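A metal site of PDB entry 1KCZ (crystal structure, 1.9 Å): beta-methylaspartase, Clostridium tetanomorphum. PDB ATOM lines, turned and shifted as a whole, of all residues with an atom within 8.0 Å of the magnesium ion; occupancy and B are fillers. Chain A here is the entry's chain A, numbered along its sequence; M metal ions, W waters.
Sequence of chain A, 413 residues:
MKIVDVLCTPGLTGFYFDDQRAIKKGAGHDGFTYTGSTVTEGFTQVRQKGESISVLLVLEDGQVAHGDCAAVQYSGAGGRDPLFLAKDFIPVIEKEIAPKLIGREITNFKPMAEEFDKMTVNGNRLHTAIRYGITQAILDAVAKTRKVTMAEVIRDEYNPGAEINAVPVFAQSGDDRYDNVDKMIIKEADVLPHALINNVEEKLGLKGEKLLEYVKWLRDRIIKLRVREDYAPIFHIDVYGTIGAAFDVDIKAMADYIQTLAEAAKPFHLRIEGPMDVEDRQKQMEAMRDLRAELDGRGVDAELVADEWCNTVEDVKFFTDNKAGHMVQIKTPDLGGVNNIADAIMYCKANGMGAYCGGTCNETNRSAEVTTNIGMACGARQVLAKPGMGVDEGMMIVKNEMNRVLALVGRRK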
ATOM      1  N   GLN A 172     -18.865 -14.424  33.484  1.00  0.00           N
ATOM      2  CA  GLN A 172     -19.824 -15.229  32.686  1.00  0.00           C
ATOM      3  C   GLN A 172     -19.631 -16.727  32.974  1.00  0.00           C
ATOM      4  O   GLN A 172     -18.501 -17.179  33.130  1.00  0.00           O
ATOM      5  CB  GLN A 172     -19.638 -14.995  31.194  1.00  0.00           C
ATOM      6  CG  GLN A 172     -20.134 -13.691  30.698  1.00  0.00           C
ATOM      7  CD  GLN A 172     -19.722 -13.471  29.255  1.00  0.00           C
ATOM      8  OE1 GLN A 172     -18.829 -14.175  28.736  1.00  0.00           O
ATOM      9  NE2 GLN A 172     -20.324 -12.455  28.610  1.00  0.00           N
ATOM     10  N   HIS A 194     -24.342 -14.317  34.023  1.00  0.00           N
ATOM     11  CA  HIS A 194     -24.671 -14.477  32.617  1.00  0.00           C
ATOM     12  C   HIS A 194     -25.663 -15.647  32.479  1.00  0.00           C
ATOM     13  O   HIS A 194     -26.801 -15.438  32.065  1.00  0.00           O
ATOM     14  CB  HIS A 194     -23.443 -14.609  31.724  1.00  0.00           C
ATOM     15  CG  HIS A 194     -23.764 -14.488  30.294  1.00  0.00           C
ATOM     16  ND1 HIS A 194     -24.217 -15.559  29.539  1.00  0.00           N
ATOM     17  CD2 HIS A 194     -23.769 -13.401  29.466  1.00  0.00           C
ATOM     18  CE1 HIS A 194     -24.470 -15.138  28.308  1.00  0.00           C
ATOM     19  NE2 HIS A 194     -24.215 -13.833  28.229  1.00  0.00           N
ATOM     20  N   LEU A 196     -26.186 -18.043  30.467  1.00  0.00           N
ATOM     21  CA  LEU A 196     -26.463 -18.619  29.145  1.00  0.00           C
ATOM     22  C   LEU A 196     -27.900 -19.187  28.998  1.00  0.00           C
ATOM     23  O   LEU A 196     -28.114 -20.363  28.742  1.00  0.00           O
ATOM     24  CB  LEU A 196     -25.377 -19.643  28.831  1.00  0.00           C
ATOM     25  CG  LEU A 196     -25.295 -20.175  27.375  1.00  0.00           C
ATOM     26  CD1 LEU A 196     -25.024 -19.056  26.375  1.00  0.00           C
ATOM     27  CD2 LEU A 196     -24.241 -21.273  27.184  1.00  0.00           C
ATOM     28  N   HIS A 236     -26.863 -10.355  36.506  1.00  0.00           N
ATOM     29  CA  HIS A 236     -26.897 -10.013  35.104  1.00  0.00           C
ATOM     30  C   HIS A 236     -27.086 -11.328  34.399  1.00  0.00           C
ATOM     31  O   HIS A 236     -26.211 -12.177  34.423  1.00  0.00           O
ATOM     32  CB  HIS A 236     -25.614  -9.295  34.736  1.00  0.00           C
ATOM     33  CG  HIS A 236     -25.455  -8.914  33.286  1.00  0.00           C
ATOM     34  ND1 HIS A 236     -25.962  -9.628  32.210  1.00  0.00           N
ATOM     35  CD2 HIS A 236     -24.763  -7.874  32.753  1.00  0.00           C
ATOM     36  CE1 HIS A 236     -25.579  -9.020  31.075  1.00  0.00           C
ATOM     37  NE2 HIS A 236     -24.870  -7.967  31.387  1.00  0.00           N
ATOM     38  N   ILE A 237     -28.265 -11.505  33.814  1.00  0.00           N
ATOM     39  CA  ILE A 237     -28.621 -12.772  33.182  1.00  0.00           C
ATOM     40  C   ILE A 237     -28.998 -12.477  31.722  1.00  0.00           C
ATOM     41  O   ILE A 237     -29.820 -11.611  31.487  1.00  0.00           O
ATOM     42  CB  ILE A 237     -29.762 -13.477  33.927  1.00  0.00           C
ATOM     43  CG1 ILE A 237     -29.201 -13.932  35.282  1.00  0.00           C
ATOM     44  CG2 ILE A 237     -30.277 -14.700  33.126  1.00  0.00           C
ATOM     45  CD1 ILE A 237     -30.244 -14.243  36.308  1.00  0.00           C
ATOM     46  N   ASP A 238     -28.376 -13.218  30.806  1.00  0.00           N
ATOM     47  CA  ASP A 238     -28.623 -13.096  29.373  1.00  0.00           C
ATOM     48  C   ASP A 238     -29.622 -14.171  28.934  1.00  0.00           C
ATOM     49  O   ASP A 238     -29.355 -15.369  29.086  1.00  0.00           O
ATOM     50  CB  ASP A 238     -27.289 -13.205  28.615  1.00  0.00           C
ATOM     51  CG  ASP A 238     -27.398 -12.770  27.143  1.00  0.00           C
ATOM     52  OD1 ASP A 238     -28.528 -12.736  26.562  1.00  0.00           O
ATOM     53  OD2 ASP A 238     -26.390 -12.415  26.484  1.00  0.00           O
ATOM     54  N   VAL A 239     -30.766 -13.742  28.447  1.00  0.00           N
ATOM     55  CA  VAL A 239     -31.855 -14.669  28.045  1.00  0.00           C
ATOM     56  C   VAL A 239     -32.016 -14.866  26.557  1.00  0.00           C
ATOM     57  O   VAL A 239     -32.993 -15.488  26.090  1.00  0.00           O
ATOM     58  CB  VAL A 239     -33.230 -14.275  28.696  1.00  0.00           C
ATOM     59  CG1 VAL A 239     -33.111 -14.292  30.202  1.00  0.00           C
ATOM     60  CG2 VAL A 239     -33.786 -12.923  28.191  1.00  0.00           C
ATOM     61  N   TYR A 240     -31.127 -14.242  25.775  1.00  0.00           N
ATOM     62  CA  TYR A 240     -31.030 -14.547  24.330  1.00  0.00           C
ATOM     63  C   TYR A 240     -32.348 -14.425  23.613  1.00  0.00           C
ATOM     64  O   TYR A 240     -32.672 -15.240  22.739  1.00  0.00           O
ATOM     65  CB  TYR A 240     -30.481 -15.989  24.176  1.00  0.00           C
ATOM     66  CG  TYR A 240     -29.045 -16.061  24.470  1.00  0.00           C
ATOM     67  CD1 TYR A 240     -28.587 -16.102  25.793  1.00  0.00           C
ATOM     68  CD2 TYR A 240     -28.103 -16.035  23.430  1.00  0.00           C
ATOM     69  CE1 TYR A 240     -27.267 -16.104  26.064  1.00  0.00           C
ATOM     70  CE2 TYR A 240     -26.710 -16.059  23.714  1.00  0.00           C
ATOM     71  CZ  TYR A 240     -26.317 -16.059  25.028  1.00  0.00           C
ATOM     72  OH  TYR A 240     -24.983 -16.051  25.361  1.00  0.00           O
ATOM     73  N   GLY A 241     -33.115 -13.426  23.995  1.00  0.00           N
ATOM     74  CA  GLY A 241     -34.440 -13.184  23.428  1.00  0.00           C
ATOM     75  C   GLY A 241     -35.561 -14.113  23.833  1.00  0.00           C
ATOM     76  O   GLY A 241     -36.701 -14.014  23.281  1.00  0.00           O
ATOM     77  N   GLU A 273     -30.158  -9.129  30.111  1.00  0.00           N
ATOM     78  CA  GLU A 273     -29.619  -8.839  28.797  1.00  0.00           C
ATOM     79  C   GLU A 273     -30.421  -9.541  27.711  1.00  0.00           C
ATOM     80  O   GLU A 273     -30.833 -10.697  27.895  1.00  0.00           O
ATOM     81  CB  GLU A 273     -28.153  -9.280  28.723  1.00  0.00           C
ATOM     82  CG  GLU A 273     -27.515  -9.028  27.366  1.00  0.00           C
ATOM     83  CD  GLU A 273     -26.055  -9.465  27.285  1.00  0.00           C
ATOM     84  OE1 GLU A 273     -25.381  -9.388  28.323  1.00  0.00           O
ATOM     85  OE2 GLU A 273     -25.595  -9.860  26.169  1.00  0.00           O
ATOM     86  N   GLY A 274     -30.696  -8.832  26.608  1.00  0.00           N
ATOM     87  CA  GLY A 274     -31.433  -9.393  25.504  1.00  0.00           C
ATOM     88  C   GLY A 274     -32.822  -9.967  25.782  1.00  0.00           C
ATOM     89  O   GLY A 274     -33.119 -11.118  25.399  1.00  0.00           O
ATOM     90  N   VAL A 305     -30.367  -4.762  29.360  1.00  0.00           N
ATOM     91  CA  VAL A 305     -29.094  -4.601  28.654  1.00  0.00           C
ATOM     92  C   VAL A 305     -29.258  -4.963  27.191  1.00  0.00           C
ATOM     93  O   VAL A 305     -29.712  -6.067  26.845  1.00  0.00           O
ATOM     94  CB  VAL A 305     -28.052  -5.472  29.236  1.00  0.00           C
ATOM     95  CG1 VAL A 305     -26.714  -5.198  28.593  1.00  0.00           C
ATOM     96  CG2 VAL A 305     -27.973  -5.284  30.729  1.00  0.00           C
ATOM     97  N   ALA A 306     -28.929  -4.021  26.314  1.00  0.00           N
ATOM     98  CA  ALA A 306     -28.978  -4.270  24.848  1.00  0.00           C
ATOM     99  C   ALA A 306     -27.834  -5.103  24.368  1.00  0.00           C
ATOM    100  O   ALA A 306     -26.693  -4.996  24.891  1.00  0.00           O
ATOM    101  CB  ALA A 306     -28.983  -2.940  24.051  1.00  0.00           C
ATOM    102  N   ASP A 307     -28.103  -5.970  23.369  1.00  0.00           N
ATOM    103  CA  ASP A 307     -27.066  -6.771  22.755  1.00  0.00           C
ATOM    104  C   ASP A 307     -27.442  -6.991  21.300  1.00  0.00           C
ATOM    105  O   ASP A 307     -26.891  -6.334  20.402  1.00  0.00           O
ATOM    106  CB  ASP A 307     -26.901  -8.103  23.482  1.00  0.00           C
ATOM    107  CG  ASP A 307     -25.860  -9.046  22.819  1.00  0.00           C
ATOM    108  OD1 ASP A 307     -25.327  -8.708  21.713  1.00  0.00           O
ATOM    109  OD2 ASP A 307     -25.556 -10.169  23.339  1.00  0.00           O
ATOM    110  N   GLU A 308     -28.379  -7.893  21.053  1.00  0.00           N
ATOM    111  CA  GLU A 308     -28.734  -8.236  19.696  1.00  0.00           C
ATOM    112  C   GLU A 308     -29.150  -6.963  18.916  1.00  0.00           C
ATOM    113  O   GLU A 308     -29.894  -6.150  19.416  1.00  0.00           O
ATOM    114  CB  GLU A 308     -29.835  -9.297  19.673  1.00  0.00           C
ATOM    115  CG  GLU A 308     -29.331 -10.711  19.994  1.00  0.00           C
ATOM    116  CD  GLU A 308     -28.956 -11.008  21.441  1.00  0.00           C
ATOM    117  OE1 GLU A 308     -29.230 -10.207  22.349  1.00  0.00           O
ATOM    118  OE2 GLU A 308     -28.418 -12.133  21.680  1.00  0.00           O
ATOM    119  N   GLN A 329     -24.222  -3.020  25.611  1.00  0.00           N
ATOM    120  CA  GLN A 329     -23.027  -3.834  25.568  1.00  0.00           C
ATOM    121  C   GLN A 329     -22.118  -3.258  24.484  1.00  0.00           C
ATOM    122  O   GLN A 329     -22.531  -3.109  23.347  1.00  0.00           O
ATOM    123  CB  GLN A 329     -23.343  -5.288  25.261  1.00  0.00           C
ATOM    124  CG  GLN A 329     -22.095  -6.121  25.303  1.00  0.00           C
ATOM    125  CD  GLN A 329     -22.291  -7.627  25.067  1.00  0.00           C
ATOM    126  OE1 GLN A 329     -21.351  -8.302  24.664  1.00  0.00           O
ATOM    127  NE2 GLN A 329     -23.473  -8.144  25.309  1.00  0.00           N
ATOM    128  N   LYS A 331     -19.099  -4.027  22.336  1.00  0.00           N
ATOM    129  CA  LYS A 331     -18.552  -5.331  21.939  1.00  0.00           C
ATOM    130  C   LYS A 331     -17.123  -5.126  21.449  1.00  0.00           C
ATOM    131  O   LYS A 331     -16.855  -4.986  20.241  1.00  0.00           O
ATOM    132  CB  LYS A 331     -19.437  -5.914  20.816  1.00  0.00           C
ATOM    133  CG  LYS A 331     -20.863  -6.139  21.279  1.00  0.00           C
ATOM    134  CD  LYS A 331     -21.816  -6.516  20.179  1.00  0.00           C
ATOM    135  CE  LYS A 331     -23.206  -6.712  20.780  1.00  0.00           C
ATOM    136  NZ  LYS A 331     -24.251  -7.125  19.802  1.00  0.00           N
ATOM    137  N   TYR A 356     -21.567  -1.096  29.169  1.00  0.00           N
ATOM    138  CA  TYR A 356     -21.017  -2.407  29.563  1.00  0.00           C
ATOM    139  C   TYR A 356     -19.856  -2.679  28.581  1.00  0.00           C
ATOM    140  O   TYR A 356     -20.075  -2.925  27.414  1.00  0.00           O
ATOM    141  CB  TYR A 356     -22.160  -3.487  29.522  1.00  0.00           C
ATOM    142  CG  TYR A 356     -21.696  -4.925  29.449  1.00  0.00           C
ATOM    143  CD1 TYR A 356     -20.445  -5.306  29.892  1.00  0.00           C
ATOM    144  CD2 TYR A 356     -22.499  -5.896  28.870  1.00  0.00           C
ATOM    145  CE1 TYR A 356     -20.027  -6.614  29.800  1.00  0.00           C
ATOM    146  CE2 TYR A 356     -22.075  -7.197  28.777  1.00  0.00           C
ATOM    147  CZ  TYR A 356     -20.867  -7.540  29.231  1.00  0.00           C
ATOM    148  OH  TYR A 356     -20.480  -8.853  29.106  1.00  0.00           O
HETATM  149 MG    MG M   1     -26.051 -11.310  24.970  1.00  0.00          MG
HETATM  150  O   HOH W   1     -24.124 -11.777  25.057  1.00  0.00           O
HETATM  151  O   HOH W   2     -26.360 -12.831  23.687  1.00  0.00           O
HETATM  152  O   HOH W   3     -28.050 -10.966  24.792  1.00  0.00           O
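Water W3 bridges OD1 of Asp 238 (2.5 Å) and OE1 of Glu 308 (2.8 Å).
O of Ile 237 sits at hydrogen-bond distance from N of Glu 273, at 2.9 Å.
A ring nitrogen (NE2) of His 236 sits close to the side-chain carboxylate of Glu 273, 3.4 Å away.
The side-chain carboxylate (OD1) of Asp 307 lies within salt-bridge range of the side-chain amino group (NZ) of Lys 331, 2.7 Å away.
The backbone NH of Val 239 is in hydrogen-bond range of the backbone carbonyl oxygen of Glu 273 (3.1 Å).
The backbone NH (N) of Asp 238 lies within hydrogen-bond range of the backbone carbonyl oxygen (O) of His 194, at 3.0 Å.
NE2 of Gln 329 sits close to OE2 of Glu 273, at 2.9 Å.
N of Tyr 240 lies within hydrogen-bond range of OD1 of Asp 238 (3.1 Å).
Three residues have an atom within 4 Å of the magnesium ion: Asp 238, Glu 273 and Asp 307.
The nearest printed residue that does not touch the magnesium ion is Gln 329 (4.1 Å).
The side-chain carboxylate (OD2) of Asp 238 is bound to the magnesium ion (1.9 Å).
OE2 of Glu 273 binds the magnesium ion, at 1.9 Å.
Water W1 is bound to the magnesium ion (2.0 Å).
The magnesium ion is bound by water W2 (2.0 Å).
The magnesium ion is bound by water W3, at 2.0 Å.
OD2 of Asp 307 binds the magnesium ion (2.1 Å).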
